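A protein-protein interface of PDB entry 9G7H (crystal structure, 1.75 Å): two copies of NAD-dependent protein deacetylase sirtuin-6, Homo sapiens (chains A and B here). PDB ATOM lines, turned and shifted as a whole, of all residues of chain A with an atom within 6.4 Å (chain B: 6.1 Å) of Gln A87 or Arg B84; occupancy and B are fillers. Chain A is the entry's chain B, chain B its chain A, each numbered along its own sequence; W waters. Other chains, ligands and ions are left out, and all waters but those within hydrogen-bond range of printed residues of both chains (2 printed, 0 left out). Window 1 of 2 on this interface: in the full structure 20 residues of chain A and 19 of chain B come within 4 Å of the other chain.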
ATOM      1  N   ALA A  52     -24.943  26.247  18.773  1.00  0.00           N
ATOM      2  CA  ALA A  52     -25.825  25.433  17.924  1.00  0.00           C
ATOM      3  C   ALA A  52     -25.626  23.928  18.192  1.00  0.00           C
ATOM      4  O   ALA A  52     -26.306  23.109  17.572  1.00  0.00           O
ATOM      5  CB  ALA A  52     -25.590  25.771  16.468  1.00  0.00           C
ATOM      6  N   SER A  53     -24.728  23.562  19.120  1.00  0.00           N
ATOM      7  CA  SER A  53     -24.571  22.196  19.611  1.00  0.00           C
ATOM      8  C   SER A  53     -25.134  22.001  21.021  1.00  0.00           C
ATOM      9  O   SER A  53     -25.001  20.910  21.577  1.00  0.00           O
ATOM     10  CB  SER A  53     -23.116  21.793  19.550  1.00  0.00           C
ATOM     11  OG  SER A  53     -22.750  21.393  18.230  1.00  0.00           O
ATOM     12  N   ARG A  84     -21.547  17.485  19.824  1.00  0.00           N
ATOM     13  CA  ARG A  84     -20.905  17.243  18.545  1.00  0.00           C
ATOM     14  C   ARG A  84     -20.373  18.568  18.001  1.00  0.00           C
ATOM     15  O   ARG A  84     -21.004  19.607  18.246  1.00  0.00           O
ATOM     16  CB  ARG A  84     -21.993  16.670  17.630  1.00  0.00           C
ATOM     17  CG  ARG A  84     -21.602  16.535  16.162  1.00  0.00           C
ATOM     18  CD  ARG A  84     -22.777  16.522  15.179  1.00  0.00           C
ATOM     19  NE  ARG A  84     -22.205  16.217  13.858  1.00  0.00           N
ATOM     20  CZ  ARG A  84     -21.538  17.076  13.079  1.00  0.00           C
ATOM     21  NH1 ARG A  84     -20.499  16.649  12.393  1.00  0.00           N
ATOM     22  NH2 ARG A  84     -21.821  18.376  13.072  1.00  0.00           N
ATOM     23  N   PRO A  85     -19.229  18.588  17.266  1.00  0.00           N
ATOM     24  CA  PRO A  85     -18.805  19.798  16.555  1.00  0.00           C
ATOM     25  C   PRO A  85     -19.876  20.300  15.590  1.00  0.00           C
ATOM     26  O   PRO A  85     -20.592  19.497  14.967  1.00  0.00           O
ATOM     27  CB  PRO A  85     -17.489  19.367  15.847  1.00  0.00           C
ATOM     28  CG  PRO A  85     -17.070  18.067  16.554  1.00  0.00           C
ATOM     29  CD  PRO A  85     -18.409  17.409  16.923  1.00  0.00           C
ATOM     30  N   THR A  86     -20.024  21.628  15.523  1.00  0.00           N
ATOM     31  CA  THR A  86     -20.943  22.334  14.644  1.00  0.00           C
ATOM     32  C   THR A  86     -20.458  22.242  13.197  1.00  0.00           C
ATOM     33  O   THR A  86     -19.324  21.898  12.915  1.00  0.00           O
ATOM     34  CB  THR A  86     -21.130  23.797  15.093  1.00  0.00           C
ATOM     35  OG1 THR A  86     -19.873  24.480  15.053  1.00  0.00           O
ATOM     36  CG2 THR A  86     -21.724  23.890  16.491  1.00  0.00           C
ATOM     37  N   GLN A  87     -21.272  22.750  12.279  1.00  0.00           N
ATOM     38  CA  GLN A  87     -20.852  22.889  10.889  1.00  0.00           C
ATOM     39  C   GLN A  87     -19.670  23.868  10.850  1.00  0.00           C
ATOM     40  O   GLN A  87     -18.760  23.670  10.062  1.00  0.00           O
ATOM     41  CB  GLN A  87     -22.066  23.321  10.072  1.00  0.00           C
ATOM     42  CG  GLN A  87     -23.253  22.370  10.193  1.00  0.00           C
ATOM     43  CD  GLN A  87     -24.538  22.934   9.636  1.00  0.00           C
ATOM     44  OE1 GLN A  87     -24.786  22.924   8.421  1.00  0.00           O
ATOM     45  NE2 GLN A  87     -25.390  23.417  10.533  1.00  0.00           N
ATOM     46  N   THR A  88     -19.667  24.864  11.757  1.00  0.00           N
ATOM     47  CA  THR A  88     -18.550  25.814  11.846  1.00  0.00           C
ATOM     48  C   THR A  88     -17.204  25.162  12.235  1.00  0.00           C
ATOM     49  O   THR A  88     -16.143  25.454  11.590  1.00  0.00           O
ATOM     50  CB  THR A  88     -18.966  26.981  12.775  1.00  0.00           C
ATOM     51  OG1 THR A  88     -19.818  27.941  12.140  1.00  0.00           O
ATOM     52  CG2 THR A  88     -17.753  27.841  13.101  1.00  0.00           C
ATOM     53  N   HIS A  89     -17.215  24.347  13.309  1.00  0.00           N
ATOM     54  CA  HIS A  89     -16.099  23.534  13.780  1.00  0.00           C
ATOM     55  C   HIS A  89     -15.548  22.745  12.605  1.00  0.00           C
ATOM     56  O   HIS A  89     -14.373  22.818  12.232  1.00  0.00           O
ATOM     57  CB  HIS A  89     -16.449  22.670  15.008  1.00  0.00           C
ATOM     58  CG  HIS A  89     -16.683  23.347  16.326  1.00  0.00           C
ATOM     59  ND1 HIS A  89     -17.943  23.770  16.674  1.00  0.00           N
ATOM     60  CD2 HIS A  89     -15.875  23.778  17.338  1.00  0.00           C
ATOM     61  CE1 HIS A  89     -17.940  24.288  17.906  1.00  0.00           C
ATOM     62  NE2 HIS A  89     -16.658  24.361  18.318  1.00  0.00           N
ATOM     63  N   MET A  90     -16.426  22.108  11.824  1.00  0.00           N
ATOM     64  CA  MET A  90     -15.976  21.207  10.771  1.00  0.00           C
ATOM     65  C   MET A  90     -15.457  21.931   9.517  1.00  0.00           C
ATOM     66  O   MET A  90     -14.600  21.400   8.807  1.00  0.00           O
ATOM     67  CB  MET A  90     -17.170  20.318  10.420  1.00  0.00           C
ATOM     68  CG  MET A  90     -17.554  19.313  11.501  1.00  0.00           C
ATOM     69  SD  MET A  90     -16.204  18.598  12.453  1.00  0.00           S
ATOM     70  CE  MET A  90     -15.268  17.685  11.236  1.00  0.00           C
ATOM     71  N   ALA A  91     -15.994  23.107   9.230  1.00  0.00           N
ATOM     72  CA  ALA A  91     -15.550  23.967   8.156  1.00  0.00           C
ATOM     73  C   ALA A  91     -14.144  24.446   8.481  1.00  0.00           C
ATOM     74  O   ALA A  91     -13.341  24.449   7.569  1.00  0.00           O
ATOM     75  CB  ALA A  91     -16.492  25.099   7.914  1.00  0.00           C
ATOM     76  N   LEU A  92     -13.857  24.769   9.748  1.00  0.00           N
ATOM     77  CA  LEU A  92     -12.511  25.224  10.103  1.00  0.00           C
ATOM     78  C   LEU A  92     -11.501  24.099   9.884  1.00  0.00           C
ATOM     79  O   LEU A  92     -10.385  24.415   9.428  1.00  0.00           O
ATOM     80  CB  LEU A  92     -12.419  25.811  11.500  1.00  0.00           C
ATOM     81  CG  LEU A  92     -13.236  27.077  11.742  1.00  0.00           C
ATOM     82  CD1 LEU A  92     -13.345  27.320  13.233  1.00  0.00           C
ATOM     83  CD2 LEU A  92     -12.708  28.281  11.009  1.00  0.00           C
ATOM     84  N   ASP A 253     -22.961  29.323  11.689  1.00  0.00           N
ATOM     85  CA  ASP A 253     -23.281  28.197  10.799  1.00  0.00           C
ATOM     86  C   ASP A 253     -23.766  28.650   9.414  1.00  0.00           C
ATOM     87  O   ASP A 253     -23.323  28.083   8.396  1.00  0.00           O
ATOM     88  CB  ASP A 253     -24.216  27.195  11.460  1.00  0.00           C
ATOM     89  CG  ASP A 253     -23.573  26.258  12.472  1.00  0.00           C
ATOM     90  OD1 ASP A 253     -22.317  26.322  12.636  1.00  0.00           O
ATOM     91  OD2 ASP A 253     -24.322  25.479  13.125  1.00  0.00           O
ATOM     92  N   GLU A 254     -24.720  29.594   9.348  1.00  0.00           N
ATOM     93  CA  GLU A 254     -25.234  30.082   8.067  1.00  0.00           C
ATOM     94  C   GLU A 254     -24.104  30.731   7.278  1.00  0.00           C
ATOM     95  O   GLU A 254     -23.890  30.453   6.086  1.00  0.00           O
ATOM     96  CB  GLU A 254     -26.438  30.962   8.423  1.00  0.00           C
ATOM     97  CG  GLU A 254     -27.192  31.556   7.249  1.00  0.00           C
ATOM     98  CD  GLU A 254     -28.224  32.587   7.688  1.00  0.00           C
ATOM     99  OE1 GLU A 254     -29.007  32.908   6.788  1.00  0.00           O
ATOM    100  OE2 GLU A 254     -28.230  33.091   8.842  1.00  0.00           O
ATOM    101  N   MET A 256     -20.670  30.456   7.710  1.00  0.00           N
ATOM    102  CA  MET A 256     -19.627  29.520   7.314  1.00  0.00           C
ATOM    103  C   MET A 256     -20.121  28.588   6.191  1.00  0.00           C
ATOM    104  O   MET A 256     -19.339  28.253   5.327  1.00  0.00           O
ATOM    105  CB  MET A 256     -19.057  28.790   8.539  1.00  0.00           C
ATOM    106  CG  MET A 256     -18.287  29.693   9.513  1.00  0.00           C
ATOM    107  SD  MET A 256     -16.865  30.483   8.735  1.00  0.00           S
ATOM    108  CE  MET A 256     -15.771  29.051   8.804  1.00  0.00           C
ATOM    109  N   THR A 257     -21.431  28.259   6.102  1.00  0.00           N
ATOM    110  CA  THR A 257     -21.914  27.316   5.098  1.00  0.00           C
ATOM    111  C   THR A 257     -21.895  27.954   3.704  1.00  0.00           C
ATOM    112  O   THR A 257     -21.438  27.348   2.738  1.00  0.00           O
ATOM    113  CB  THR A 257     -23.280  26.683   5.415  1.00  0.00           C
ATOM    114  OG1 THR A 257     -24.222  27.665   5.806  1.00  0.00           O
ATOM    115  CG2 THR A 257     -23.265  25.682   6.559  1.00  0.00           C
ATOM    116  N   ILE A 267     -18.043  20.534   3.582  1.00  0.00           N
ATOM    117  CA  ILE A 267     -17.853  20.446   5.024  1.00  0.00           C
ATOM    118  C   ILE A 267     -17.782  18.956   5.349  1.00  0.00           C
ATOM    119  O   ILE A 267     -18.700  18.202   5.054  1.00  0.00           O
ATOM    120  CB  ILE A 267     -18.915  21.221   5.835  1.00  0.00           C
ATOM    121  CG1 ILE A 267     -18.904  22.742   5.476  1.00  0.00           C
ATOM    122  CG2 ILE A 267     -18.690  21.002   7.337  1.00  0.00           C
ATOM    123  CD1 ILE A 267     -19.928  23.603   6.202  1.00  0.00           C
ATOM    124  N   SER B  53     -29.641  20.871  18.392  1.00  0.00           N
ATOM    125  CA  SER B  53     -29.337  21.596  17.141  1.00  0.00           C
ATOM    126  C   SER B  53     -29.609  23.120  17.189  1.00  0.00           C
ATOM    127  O   SER B  53     -29.449  23.778  16.170  1.00  0.00           O
ATOM    128  CB  SER B  53     -30.109  20.978  16.002  1.00  0.00           C
ATOM    129  OG  SER B  53     -29.543  19.709  15.672  1.00  0.00           O
ATOM    130  N   THR B  78     -30.004  28.804  15.691  1.00  0.00           N
ATOM    131  CA  THR B  78     -29.976  28.504  14.266  1.00  0.00           C
ATOM    132  C   THR B  78     -31.300  28.972  13.671  1.00  0.00           C
ATOM    133  O   THR B  78     -32.266  29.131  14.408  1.00  0.00           O
ATOM    134  CB  THR B  78     -29.797  26.988  14.055  1.00  0.00           C
ATOM    135  OG1 THR B  78     -29.582  26.688  12.689  1.00  0.00           O
ATOM    136  CG2 THR B  78     -31.064  26.196  14.371  1.00  0.00           C
ATOM    137  N   SER B  82     -30.743  26.502   8.443  1.00  0.00           N
ATOM    138  CA  SER B  82     -29.346  26.202   8.792  1.00  0.00           C
ATOM    139  C   SER B  82     -29.158  25.124   9.866  1.00  0.00           C
ATOM    140  O   SER B  82     -28.018  24.785  10.207  1.00  0.00           O
ATOM    141  CB  SER B  82     -28.611  27.451   9.160  1.00  0.00           C
ATOM    142  OG  SER B  82     -28.534  28.317   8.039  1.00  0.00           O
ATOM    143  N   ALA B  83     -30.255  24.579  10.380  1.00  0.00           N
ATOM    144  CA  ALA B  83     -30.223  23.553  11.429  1.00  0.00           C
ATOM    145  C   ALA B  83     -29.708  22.231  10.873  1.00  0.00           C
ATOM    146  O   ALA B  83     -30.100  21.858   9.760  1.00  0.00           O
ATOM    147  CB  ALA B  83     -31.601  23.394  12.010  1.00  0.00           C
ATOM    148  N   ARG B  84     -28.848  21.546  11.626  1.00  0.00           N
ATOM    149  CA  ARG B  84     -28.348  20.239  11.231  1.00  0.00           C
ATOM    150  C   ARG B  84     -29.073  19.176  12.054  1.00  0.00           C
ATOM    151  O   ARG B  84     -29.401  19.417  13.234  1.00  0.00           O
ATOM    152  CB  ARG B  84     -26.820  20.208  11.360  1.00  0.00           C
ATOM    153  CG  ARG B  84     -26.218  19.968  12.732  1.00  0.00           C
ATOM    154  CD  ARG B  84     -24.974  19.108  12.600  1.00  0.00           C
ATOM    155  NE  ARG B  84     -25.322  17.707  12.346  1.00  0.00           N
ATOM    156  CZ  ARG B  84     -24.741  16.893  11.484  1.00  0.00           C
ATOM    157  NH1 ARG B  84     -23.759  17.331  10.706  1.00  0.00           N
ATOM    158  NH2 ARG B  84     -25.140  15.633  11.406  1.00  0.00           N
ATOM    159  N   PRO B  85     -29.431  18.012  11.477  1.00  0.00           N
ATOM    160  CA  PRO B  85     -30.003  16.920  12.263  1.00  0.00           C
ATOM    161  C   PRO B  85     -29.021  16.501  13.351  1.00  0.00           C
ATOM    162  O   PRO B  85     -27.797  16.474  13.131  1.00  0.00           O
ATOM    163  CB  PRO B  85     -30.242  15.858  11.201  1.00  0.00           C
ATOM    164  CG  PRO B  85     -30.374  16.636   9.929  1.00  0.00           C
ATOM    165  CD  PRO B  85     -29.266  17.669  10.071  1.00  0.00           C
ATOM    166  N   THR B  86     -29.557  16.164  14.506  1.00  0.00           N
ATOM    167  CA  THR B  86     -28.794  15.718  15.670  1.00  0.00           C
ATOM    168  C   THR B  86     -28.276  14.298  15.472  1.00  0.00           C
ATOM    169  O   THR B  86     -28.657  13.639  14.507  1.00  0.00           O
ATOM    170  CB  THR B  86     -29.663  15.794  16.925  1.00  0.00           C
ATOM    171  OG1 THR B  86     -30.697  14.818  16.787  1.00  0.00           O
ATOM    172  CG2 THR B  86     -30.227  17.176  17.159  1.00  0.00           C
ATOM    173  N   GLN B  87     -27.421  13.850  16.405  1.00  0.00           N
ATOM    174  CA  GLN B  87     -26.934  12.483  16.459  1.00  0.00           C
ATOM    175  C   GLN B  87     -28.172  11.588  16.563  1.00  0.00           C
ATOM    176  O   GLN B  87     -28.250  10.598  15.869  1.00  0.00           O
ATOM    177  CB  GLN B  87     -25.903  12.240  17.555  1.00  0.00           C
ATOM    178  CG  GLN B  87     -24.688  13.163  17.429  1.00  0.00           C
ATOM    179  CD  GLN B  87     -23.725  13.085  18.615  1.00  0.00           C
ATOM    180  OE1 GLN B  87     -22.956  12.129  18.800  1.00  0.00           O
ATOM    181  NE2 GLN B  87     -23.776  14.096  19.477  1.00  0.00           N
ATOM    182  N   HIS B  89     -31.450  12.185  15.404  1.00  0.00           N
ATOM    183  CA  HIS B  89     -32.071  12.115  14.085  1.00  0.00           C
ATOM    184  C   HIS B  89     -31.328  11.111  13.188  1.00  0.00           C
ATOM    185  O   HIS B  89     -31.907  10.274  12.531  1.00  0.00           O
ATOM    186  CB  HIS B  89     -32.080  13.484  13.443  1.00  0.00           C
ATOM    187  CG  HIS B  89     -33.017  14.498  13.940  1.00  0.00           C
ATOM    188  ND1 HIS B  89     -32.627  15.396  14.883  1.00  0.00           N
ATOM    189  CD2 HIS B  89     -34.305  14.766  13.654  1.00  0.00           C
ATOM    190  CE1 HIS B  89     -33.605  16.236  15.109  1.00  0.00           C
ATOM    191  NE2 HIS B  89     -34.689  15.822  14.379  1.00  0.00           N
ATOM    192  N   MET B  90     -30.002  11.205  13.118  1.00  0.00           N
ATOM    193  CA  MET B  90     -29.200  10.313  12.248  1.00  0.00           C
ATOM    194  C   MET B  90     -29.180   8.852  12.750  1.00  0.00           C
ATOM    195  O   MET B  90     -29.111   7.959  11.915  1.00  0.00           O
ATOM    196  CB  MET B  90     -27.771  10.879  12.086  1.00  0.00           C
ATOM    197  CG  MET B  90     -27.689  12.211  11.401  1.00  0.00           C
ATOM    198  SD  MET B  90     -28.767  12.446   9.961  1.00  0.00           S
ATOM    199  CE  MET B  90     -28.013  11.355   8.764  1.00  0.00           C
ATOM    200  N   LEU B 112     -36.636  18.471  10.124  1.00  0.00           N
ATOM    201  CA  LEU B 112     -35.326  17.798  10.242  1.00  0.00           C
ATOM    202  C   LEU B 112     -35.310  16.292   9.951  1.00  0.00           C
ATOM    203  O   LEU B 112     -34.287  15.792   9.479  1.00  0.00           O
ATOM    204  CB  LEU B 112     -34.735  18.074  11.627  1.00  0.00           C
ATOM    205  CG  LEU B 112     -34.086  19.455  11.842  1.00  0.00           C
ATOM    206  CD1 LEU B 112     -33.745  19.649  13.286  1.00  0.00           C
ATOM    207  CD2 LEU B 112     -32.860  19.649  10.969  1.00  0.00           C
ATOM    208  N   PRO B 268     -24.822   7.271  10.822  1.00  0.00           N
ATOM    209  CA  PRO B 268     -24.405   7.712   9.476  1.00  0.00           C
ATOM    210  C   PRO B 268     -24.154   9.218   9.299  1.00  0.00           C
ATOM    211  O   PRO B 268     -24.789  10.040   9.952  1.00  0.00           O
ATOM    212  CB  PRO B 268     -25.566   7.253   8.584  1.00  0.00           C
ATOM    213  CG  PRO B 268     -26.758   7.155   9.513  1.00  0.00           C
ATOM    214  CD  PRO B 268     -26.182   6.705  10.852  1.00  0.00           C
ATOM    215  N   ALA B 269     -23.275   9.597   8.363  1.00  0.00           N
ATOM    216  CA  ALA B 269     -22.927  10.987   8.100  1.00  0.00           C
ATOM    217  C   ALA B 269     -24.091  11.701   7.397  1.00  0.00           C
ATOM    218  O   ALA B 269     -24.935  11.063   6.752  1.00  0.00           O
ATOM    219  CB  ALA B 269     -21.637  11.033   7.282  1.00  0.00           C
ATOM    220  N   TRP B 270     -24.216  13.010   7.610  1.00  0.00           N
ATOM    221  CA  TRP B 270     -25.301  13.762   6.991  1.00  0.00           C
ATOM    222  C   TRP B 270     -24.776  14.414   5.723  1.00  0.00           C
ATOM    223  O   TRP B 270     -23.893  15.264   5.794  1.00  0.00           O
ATOM    224  CB  TRP B 270     -25.895  14.802   7.963  1.00  0.00           C
ATOM    225  CG  TRP B 270     -27.104  15.523   7.446  1.00  0.00           C
ATOM    226  CD1 TRP B 270     -28.276  14.971   6.990  1.00  0.00           C
ATOM    227  CD2 TRP B 270     -27.269  16.953   7.340  1.00  0.00           C
ATOM    228  NE1 TRP B 270     -29.131  15.962   6.597  1.00  0.00           N
ATOM    229  CE2 TRP B 270     -28.549  17.184   6.808  1.00  0.00           C
ATOM    230  CE3 TRP B 270     -26.457  18.058   7.652  1.00  0.00           C
ATOM    231  CZ2 TRP B 270     -29.051  18.471   6.596  1.00  0.00           C
ATOM    232  CZ3 TRP B 270     -26.942  19.320   7.421  1.00  0.00           C
ATOM    233  CH2 TRP B 270     -28.219  19.527   6.900  1.00  0.00           C
HETATM  234  O   HOH W   1     -26.754  25.340  12.746  1.00  0.00           O
HETATM  235  O   HOH W   2     -30.498  30.406   7.288  1.00  0.00           O
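The side-chain hydroxyl (OG) of Ser B53 sits at hydrogen-bond distance from the backbone carbonyl oxygen (O) of Arg B84. OG1 of Thr B78 sits close to O of Ser B82, at 3.5 Å. O of Arg A84 lies within hydrogen-bond range of OG of Ser A53, at 2.5 Å. The side-chain amide nitrogen (NE2) of Gln A87 is in hydrogen-bond range of the side-chain carboxylate (OD2) of Asp A253 (3.5 Å). The backbone carbonyl oxygen (O) of Glu A254 lies within hydrogen-bond range of the side-chain hydroxyl (OG1) of Thr A257 (2.8 Å).
Arg B84 touches its own counterpart, Arg A84. Arg A84 touches Gln B87, and with the chains exchanged Gln A87 touches Arg B84.
Printed residues of chain A that touch a printed residue of chain B: Ala A52, Arg A84, Gln A87 and Glu A254. Of the 14 printed residues of chain B, 4 touch a printed residue of chain A. Along chain B the printed residues that touch a printed residue of chain A span positions 53 to 87. Among the printed residues, 6 pairs touch across the chains. Among the printed residues, no Asp or Glu carboxylate lies within 4 Å of a Lys or Arg side-chain nitrogen of the other chain.
Printed residues of chain B within 4 Å of Ala A52: Ser B53. Of the printed residues of chain B, Arg A84 touches Arg B84 and Gln B87. Printed residues of chain B within 4 Å of Glu A254: Ser B82 (3.4 Å). Of the printed residues of chain A, Ser B82 touches Gln A87 and Glu A254. Of chain A, only Arg A84 (3.2 Å) and Gln A87 (3.6 Å) come within 4 Å of Arg B84. The nearest residue of chain B that does not touch Gln A87 is Trp B270 (4.3 Å).
Water W1 lies within hydrogen-bond range of OD2 of Asp A253 (2.5 Å), O of Ser B82 (2.9 Å), OG1 of Thr B78 (3.1 Å) and NE2 of Gln A87 (3.2 Å). Water W2 lies within hydrogen-bond range of the side-chain carboxylate (OE1) of Glu A254 and the side-chain hydroxyl (OG) of Ser B82.
The backbone carbonyl oxygen (O) of Ser B82 is in hydrogen-bond range of the side-chain amide nitrogen (NE2) of Gln A87 (3.0 Å). The guanidinium group of Arg B84 lies close to the guanidinium group of Arg A84, at 3.2 Å.
Ser B53 touches Ala A52 (C to O, 3.3 Å). Gln B87 touches Arg A84. Arg B84 touches Gln A87. Glu A254 touches Ser B82.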
